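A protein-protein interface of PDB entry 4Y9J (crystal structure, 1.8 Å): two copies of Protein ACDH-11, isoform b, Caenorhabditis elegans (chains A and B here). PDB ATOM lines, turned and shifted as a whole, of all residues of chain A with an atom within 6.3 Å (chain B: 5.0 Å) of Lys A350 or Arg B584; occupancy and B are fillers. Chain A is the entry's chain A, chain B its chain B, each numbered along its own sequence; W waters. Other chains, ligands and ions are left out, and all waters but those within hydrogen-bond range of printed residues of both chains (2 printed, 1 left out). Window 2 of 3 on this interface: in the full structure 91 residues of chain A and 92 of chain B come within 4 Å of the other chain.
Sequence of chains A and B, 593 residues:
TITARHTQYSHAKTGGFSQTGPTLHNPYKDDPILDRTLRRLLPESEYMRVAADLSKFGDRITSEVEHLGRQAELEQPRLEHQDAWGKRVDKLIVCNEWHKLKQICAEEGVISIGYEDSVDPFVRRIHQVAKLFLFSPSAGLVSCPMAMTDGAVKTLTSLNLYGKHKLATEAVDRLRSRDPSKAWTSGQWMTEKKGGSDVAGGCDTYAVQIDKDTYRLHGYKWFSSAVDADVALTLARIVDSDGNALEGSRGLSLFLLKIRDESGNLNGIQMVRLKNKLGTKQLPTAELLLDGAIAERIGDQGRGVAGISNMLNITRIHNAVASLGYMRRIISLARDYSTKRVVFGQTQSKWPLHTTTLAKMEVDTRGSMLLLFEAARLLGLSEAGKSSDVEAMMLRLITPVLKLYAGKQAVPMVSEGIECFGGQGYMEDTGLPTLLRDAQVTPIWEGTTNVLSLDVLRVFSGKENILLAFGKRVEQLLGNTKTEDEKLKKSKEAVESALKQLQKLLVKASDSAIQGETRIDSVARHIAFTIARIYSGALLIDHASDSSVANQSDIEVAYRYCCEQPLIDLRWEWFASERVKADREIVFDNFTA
The backbone carbonyl oxygen (O) of Lys A350 is in hydrogen-bond range of the guanidinium group (NH2) of Arg B584 (3.0 Å).
Printed residues of chain A that touch a printed residue of chain B: Ser A338, Ser A349, Lys A350, Pro A352, Thr A355 and Ala A359. Hydrophobic or aromatic side chains of chain A within 4 Å of the printed part of chain B: Pro A352 and Ala A359. Along chain A the printed residues that touch a printed residue of chain B span positions 338 to 359. Of the 10 printed residues of chain B, 4 touch a printed residue of chain A. Hydrophobic or aromatic side chains of chain B within 4 Å of the printed part of chain A: Val B580, Val B587 and Phe B588. Among the printed residues, 6 pairs touch across the chains. Among the printed residues, no Asp or Glu carboxylate lies within 4 Å of a Lys or Arg side-chain nitrogen of the other chain.
Printed residues of chain B within 4 Å of Ser A338: Phe B588. Of the printed residues of chain B, Lys A350 touches Arg B584 (3.0 Å). Printed residues of chain B within 4 Å of Ala A359: Val B587 (3.5 Å). Of the printed residues of chain A, Val B580 touches Pro A352. Of chain A, only Lys A350 comes within 4 Å of Arg B584. Of the printed residues of chain A, Phe B588 touches Ser A338 (3.4 Å) and Ser A349 (3.8 Å). The nearest printed residue of chain B that does not touch Lys A350 is Val B580 (5.6 Å).
Water W1 lies within hydrogen-bond range of OD2 of Asp B583, OG1 of Thr A355 and O of Pro A352. Water W2 lies within hydrogen-bond range of O of Ser A349 and NE of Arg B584.
Among the printed residues, pairs that only touch across the chains: Ser A338 with Phe B588 (3.4 Å), Ser A349 with Phe B588 (3.8 Å), Pro A352 with Val B580 (3.7 Å), Thr A355 with Val B587 (3.7 Å) and Ala A359 with Val B587 (3.5 Å).
The backbone NH of Gln A348 is in hydrogen-bond range of the backbone carbonyl oxygen of Ser A338 (3.3 Å). The side-chain hydroxyl (OG1) of Thr A347 is in hydrogen-bond range of the side-chain hydroxyl (OG) of Ser A349. The backbone NH (N) of Ser A349 lies within hydrogen-bond range of the backbone carbonyl oxygen (O) of Ser A338, at 2.9 Å. The backbone carbonyl oxygen (O) of Pro A352 is in hydrogen-bond range of the side-chain hydroxyl (OG1) of Thr A355 (3.4 Å).
No position is printed for both chains.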
ATOM      1  N   SER A 338       7.598 -12.671  23.320  1.00  0.00           N
ATOM      2  CA  SER A 338       7.773 -12.299  24.715  1.00  0.00           C
ATOM      3  C   SER A 338       6.468 -12.397  25.484  1.00  0.00           C
ATOM      4  O   SER A 338       6.454 -12.581  26.717  1.00  0.00           O
ATOM      5  CB  SER A 338       8.399 -10.932  24.873  1.00  0.00           C
ATOM      6  OG  SER A 338       7.396  -9.916  24.798  1.00  0.00           O
ATOM      7  N   GLN A 346       6.808 -16.131  34.784  1.00  0.00           N
ATOM      8  CA  GLN A 346       5.997 -15.184  34.035  1.00  0.00           C
ATOM      9  C   GLN A 346       6.532 -15.008  32.643  1.00  0.00           C
ATOM     10  O   GLN A 346       7.642 -15.496  32.329  1.00  0.00           O
ATOM     11  CB  GLN A 346       5.905 -13.874  34.780  1.00  0.00           C
ATOM     12  CG  GLN A 346       7.207 -13.153  34.931  1.00  0.00           C
ATOM     13  CD  GLN A 346       7.022 -11.917  35.732  1.00  0.00           C
ATOM     14  OE1 GLN A 346       5.881 -11.584  36.104  1.00  0.00           O
ATOM     15  NE2 GLN A 346       8.117 -11.179  35.968  1.00  0.00           N
ATOM     16  N   THR A 347       5.734 -14.392  31.764  1.00  0.00           N
ATOM     17  CA  THR A 347       6.154 -14.258  30.388  1.00  0.00           C
ATOM     18  C   THR A 347       7.338 -13.336  30.334  1.00  0.00           C
ATOM     19  O   THR A 347       7.485 -12.487  31.215  1.00  0.00           O
ATOM     20  CB  THR A 347       5.009 -13.806  29.448  1.00  0.00           C
ATOM     21  OG1 THR A 347       4.452 -12.573  29.956  1.00  0.00           O
ATOM     22  CG2 THR A 347       3.917 -14.876  29.421  1.00  0.00           C
ATOM     23  N   GLN A 348       8.204 -13.541  29.341  1.00  0.00           N
ATOM     24  CA  GLN A 348       9.408 -12.684  29.170  1.00  0.00           C
ATOM     25  C   GLN A 348       9.053 -11.212  29.158  1.00  0.00           C
ATOM     26  O   GLN A 348       9.858 -10.357  29.545  1.00  0.00           O
ATOM     27  CB  GLN A 348      10.081 -12.939  27.826  1.00  0.00           C
ATOM     28  CG  GLN A 348      10.607 -14.334  27.572  1.00  0.00           C
ATOM     29  CD  GLN A 348      11.082 -14.480  26.148  1.00  0.00           C
ATOM     30  OE1 GLN A 348      10.442 -14.021  25.180  1.00  0.00           O
ATOM     31  NE2 GLN A 348      12.214 -15.132  25.992  1.00  0.00           N
ATOM     32  N   SER A 349       7.871 -10.929  28.595  1.00  0.00           N
ATOM     33  CA  SER A 349       7.378  -9.516  28.504  1.00  0.00           C
ATOM     34  C   SER A 349       7.321  -8.801  29.830  1.00  0.00           C
ATOM     35  O   SER A 349       7.372  -7.572  29.870  1.00  0.00           O
ATOM     36  CB  SER A 349       5.991  -9.462  27.877  1.00  0.00           C
ATOM     37  OG  SER A 349       5.032 -10.207  28.620  1.00  0.00           O
ATOM     38  N   LYS A 350       7.218  -9.539  30.928  1.00  0.00           N
ATOM     39  CA  LYS A 350       7.072  -8.929  32.237  1.00  0.00           C
ATOM     40  C   LYS A 350       8.381  -8.715  32.976  1.00  0.00           C
ATOM     41  O   LYS A 350       8.391  -8.084  34.043  1.00  0.00           O
ATOM     42  CB  LYS A 350       6.265  -9.843  33.141  1.00  0.00           C
ATOM     43  CG  LYS A 350       4.853 -10.098  32.727  1.00  0.00           C
ATOM     44  CD  LYS A 350       4.087  -8.875  32.376  1.00  0.00           C
ATOM     45  CE  LYS A 350       2.632  -9.005  32.813  1.00  0.00           C
ATOM     46  NZ  LYS A 350       2.237 -10.435  32.715  1.00  0.00           N
ATOM     47  N   TRP A 351       9.480  -9.285  32.474  1.00  0.00           N
ATOM     48  CA  TRP A 351      10.816  -9.170  33.144  1.00  0.00           C
ATOM     49  C   TRP A 351      11.504  -7.901  32.693  1.00  0.00           C
ATOM     50  O   TRP A 351      11.701  -7.736  31.464  1.00  0.00           O
ATOM     51  CB  TRP A 351      11.679 -10.380  32.769  1.00  0.00           C
ATOM     52  CG  TRP A 351      11.271 -11.545  33.434  1.00  0.00           C
ATOM     53  CD1 TRP A 351      10.740 -12.659  32.868  1.00  0.00           C
ATOM     54  CD2 TRP A 351      11.331 -11.784  34.855  1.00  0.00           C
ATOM     55  NE1 TRP A 351      10.472 -13.581  33.872  1.00  0.00           N
ATOM     56  CE2 TRP A 351      10.818 -13.057  35.081  1.00  0.00           C
ATOM     57  CE3 TRP A 351      11.762 -11.023  35.946  1.00  0.00           C
ATOM     58  CZ2 TRP A 351      10.736 -13.610  36.352  1.00  0.00           C
ATOM     59  CZ3 TRP A 351      11.654 -11.557  37.224  1.00  0.00           C
ATOM     60  CH2 TRP A 351      11.176 -12.853  37.402  1.00  0.00           C
ATOM     61  N   PRO A 352      11.775  -6.963  33.614  1.00  0.00           N
ATOM     62  CA  PRO A 352      12.329  -5.673  33.178  1.00  0.00           C
ATOM     63  C   PRO A 352      13.634  -5.798  32.380  1.00  0.00           C
ATOM     64  O   PRO A 352      13.896  -4.991  31.479  1.00  0.00           O
ATOM     65  CB  PRO A 352      12.619  -4.948  34.487  1.00  0.00           C
ATOM     66  CG  PRO A 352      11.691  -5.535  35.470  1.00  0.00           C
ATOM     67  CD  PRO A 352      11.429  -6.948  35.051  1.00  0.00           C
ATOM     68  N   HIS A 354      14.399  -8.032  30.188  1.00  0.00           N
ATOM     69  CA  HIS A 354      14.007  -8.330  28.857  1.00  0.00           C
ATOM     70  C   HIS A 354      13.536  -7.090  28.083  1.00  0.00           C
ATOM     71  O   HIS A 354      13.957  -6.852  26.944  1.00  0.00           O
ATOM     72  CB  HIS A 354      12.951  -9.428  28.827  1.00  0.00           C
ATOM     73  CG  HIS A 354      12.947 -10.170  27.543  1.00  0.00           C
ATOM     74  ND1 HIS A 354      11.950 -10.048  26.590  1.00  0.00           N
ATOM     75  CD2 HIS A 354      13.797 -11.109  27.078  1.00  0.00           C
ATOM     76  CE1 HIS A 354      12.216 -10.855  25.586  1.00  0.00           C
ATOM     77  NE2 HIS A 354      13.350 -11.471  25.844  1.00  0.00           N
ATOM     78  N   THR A 355      12.660  -6.310  28.690  1.00  0.00           N
ATOM     79  CA  THR A 355      12.141  -5.087  28.037  1.00  0.00           C
ATOM     80  C   THR A 355      13.203  -3.971  27.931  1.00  0.00           C
ATOM     81  O   THR A 355      13.177  -3.172  27.006  1.00  0.00           O
ATOM     82  CB  THR A 355      10.792  -4.622  28.644  1.00  0.00           C
ATOM     83  OG1 THR A 355      10.850  -4.626  30.080  1.00  0.00           O
ATOM     84  CG2 THR A 355       9.730  -5.599  28.201  1.00  0.00           C
ATOM     85  N   ALA A 359      13.907  -2.421  24.522  1.00  0.00           N
ATOM     86  CA  ALA A 359      13.633  -0.990  24.386  1.00  0.00           C
ATOM     87  C   ALA A 359      14.784  -0.279  23.692  1.00  0.00           C
ATOM     88  O   ALA A 359      14.557   0.572  22.837  1.00  0.00           O
ATOM     89  CB  ALA A 359      13.323  -0.333  25.744  1.00  0.00           C
ATOM     90  N   VAL B 580      10.725   1.094  33.953  1.00  0.00           N
ATOM     91  CA  VAL B 580      10.139  -0.149  33.360  1.00  0.00           C
ATOM     92  C   VAL B 580       8.841   0.174  32.613  1.00  0.00           C
ATOM     93  O   VAL B 580       8.599  -0.326  31.508  1.00  0.00           O
ATOM     94  CB  VAL B 580       9.847  -1.250  34.420  1.00  0.00           C
ATOM     95  CG1 VAL B 580       9.262  -2.541  33.767  1.00  0.00           C
ATOM     96  CG2 VAL B 580      11.140  -1.567  35.105  1.00  0.00           C
ATOM     97  N   LYS B 581       8.012   1.021  33.195  1.00  0.00           N
ATOM     98  CA  LYS B 581       6.755   1.378  32.567  1.00  0.00           C
ATOM     99  C   LYS B 581       6.973   2.042  31.194  1.00  0.00           C
ATOM    100  O   LYS B 581       6.257   1.755  30.199  1.00  0.00           O
ATOM    101  CB  LYS B 581       5.970   2.278  33.491  1.00  0.00           C
ATOM    102  CG  LYS B 581       4.713   2.873  32.846  1.00  0.00           C
ATOM    103  CD  LYS B 581       3.802   3.619  33.832  1.00  0.00           C
ATOM    104  CE  LYS B 581       2.632   4.322  33.119  1.00  0.00           C
ATOM    105  NZ  LYS B 581       3.015   5.107  31.894  1.00  0.00           N
ATOM    106  N   ALA B 582       8.005   2.870  31.134  1.00  0.00           N
ATOM    107  CA  ALA B 582       8.410   3.549  29.908  1.00  0.00           C
ATOM    108  C   ALA B 582       8.982   2.572  28.938  1.00  0.00           C
ATOM    109  O   ALA B 582       8.731   2.705  27.786  1.00  0.00           O
ATOM    110  CB  ALA B 582       9.410   4.676  30.191  1.00  0.00           C
ATOM    111  N   ASP B 583       9.800   1.640  29.396  1.00  0.00           N
ATOM    112  CA  ASP B 583      10.335   0.573  28.525  1.00  0.00           C
ATOM    113  C   ASP B 583       9.174  -0.166  27.885  1.00  0.00           C
ATOM    114  O   ASP B 583       9.211  -0.432  26.706  1.00  0.00           O
ATOM    115  CB  ASP B 583      11.261  -0.442  29.223  1.00  0.00           C
ATOM    116  CG  ASP B 583      12.519   0.191  29.853  1.00  0.00           C
ATOM    117  OD1 ASP B 583      12.973   1.264  29.432  1.00  0.00           O
ATOM    118  OD2 ASP B 583      13.042  -0.377  30.875  1.00  0.00           O
ATOM    119  N   ARG B 584       8.163  -0.553  28.648  1.00  0.00           N
ATOM    120  CA  ARG B 584       7.047  -1.349  28.070  1.00  0.00           C
ATOM    121  C   ARG B 584       6.251  -0.560  27.018  1.00  0.00           C
ATOM    122  O   ARG B 584       5.845  -1.081  25.984  1.00  0.00           O
ATOM    123  CB  ARG B 584       6.134  -1.847  29.189  1.00  0.00           C
ATOM    124  CG  ARG B 584       6.858  -2.826  30.122  1.00  0.00           C
ATOM    125  CD  ARG B 584       6.023  -3.112  31.350  1.00  0.00           C
ATOM    126  NE  ARG B 584       6.640  -4.156  32.129  1.00  0.00           N
ATOM    127  CZ  ARG B 584       6.268  -4.483  33.347  1.00  0.00           C
ATOM    128  NH1 ARG B 584       5.292  -3.836  33.937  1.00  0.00           N
ATOM    129  NH2 ARG B 584       6.896  -5.447  34.000  1.00  0.00           N
ATOM    130  N   GLU B 585       6.054   0.733  27.274  1.00  0.00           N
ATOM    131  CA  GLU B 585       5.353   1.554  26.390  1.00  0.00           C
ATOM    132  C   GLU B 585       6.109   1.758  25.086  1.00  0.00           C
ATOM    133  O   GLU B 585       5.490   1.770  24.014  1.00  0.00           O
ATOM    134  CB  GLU B 585       5.103   2.916  27.057  1.00  0.00           C
ATOM    135  CG  GLU B 585       3.839   3.005  27.819  1.00  0.00           C
ATOM    136  CD  GLU B 585       3.679   4.412  28.320  1.00  0.00           C
ATOM    137  OE1 GLU B 585       4.000   5.388  27.547  1.00  0.00           O
ATOM    138  OE2 GLU B 585       3.275   4.499  29.501  1.00  0.00           O
ATOM    139  N   ILE B 586       7.429   1.845  25.150  1.00  0.00           N
ATOM    140  CA  ILE B 586       8.256   1.879  23.931  1.00  0.00           C
ATOM    141  C   ILE B 586       8.163   0.557  23.136  1.00  0.00           C
ATOM    142  O   ILE B 586       8.030   0.523  21.910  1.00  0.00           O
ATOM    143  CB  ILE B 586       9.693   2.219  24.316  1.00  0.00           C
ATOM    144  CG1 ILE B 586       9.862   3.670  24.696  1.00  0.00           C
ATOM    145  CG2 ILE B 586      10.704   1.944  23.248  1.00  0.00           C
ATOM    146  CD1 ILE B 586      11.291   3.891  25.234  1.00  0.00           C
ATOM    147  N   VAL B 587       8.364  -0.546  23.832  1.00  0.00           N
ATOM    148  CA  VAL B 587       8.433  -1.833  23.205  1.00  0.00           C
ATOM    149  C   VAL B 587       7.070  -2.248  22.578  1.00  0.00           C
ATOM    150  O   VAL B 587       7.064  -2.852  21.527  1.00  0.00           O
ATOM    151  CB  VAL B 587       8.930  -2.901  24.208  1.00  0.00           C
ATOM    152  CG1 VAL B 587       8.810  -4.293  23.621  1.00  0.00           C
ATOM    153  CG2 VAL B 587      10.378  -2.620  24.578  1.00  0.00           C
ATOM    154  N   PHE B 588       5.996  -2.048  23.277  1.00  0.00           N
ATOM    155  CA  PHE B 588       4.650  -2.561  22.897  1.00  0.00           C
ATOM    156  C   PHE B 588       3.718  -1.598  22.162  1.00  0.00           C
ATOM    157  O   PHE B 588       2.502  -1.823  22.030  1.00  0.00           O
ATOM    158  CB  PHE B 588       3.999  -3.214  24.117  1.00  0.00           C
ATOM    159  CG  PHE B 588       4.731  -4.455  24.515  1.00  0.00           C
ATOM    160  CD1 PHE B 588       4.606  -5.578  23.736  1.00  0.00           C
ATOM    161  CD2 PHE B 588       5.588  -4.490  25.620  1.00  0.00           C
ATOM    162  CE1 PHE B 588       5.297  -6.719  24.058  1.00  0.00           C
ATOM    163  CE2 PHE B 588       6.258  -5.614  25.956  1.00  0.00           C
ATOM    164  CZ  PHE B 588       6.135  -6.742  25.164  1.00  0.00           C
ATOM    165  N   ASP B 589       4.317  -0.526  21.656  1.00  0.00           N
ATOM    166  CA  ASP B 589       3.608   0.526  20.933  1.00  0.00           C
ATOM    167  C   ASP B 589       2.958  -0.105  19.660  1.00  0.00           C
ATOM    168  O   ASP B 589       3.667  -0.766  18.872  1.00  0.00           O
ATOM    169  CB  ASP B 589       4.644   1.606  20.530  1.00  0.00           C
ATOM    170  CG  ASP B 589       4.010   2.901  19.964  1.00  0.00           C
ATOM    171  OD1 ASP B 589       2.795   3.117  20.052  1.00  0.00           O
ATOM    172  OD2 ASP B 589       4.777   3.726  19.434  1.00  0.00           O
HETATM  173  O   HOH W   1      12.188  -2.776  31.383  1.00  0.00           O
HETATM  174  O   HOH W   2       5.007  -5.945  30.006  1.00  0.00           O
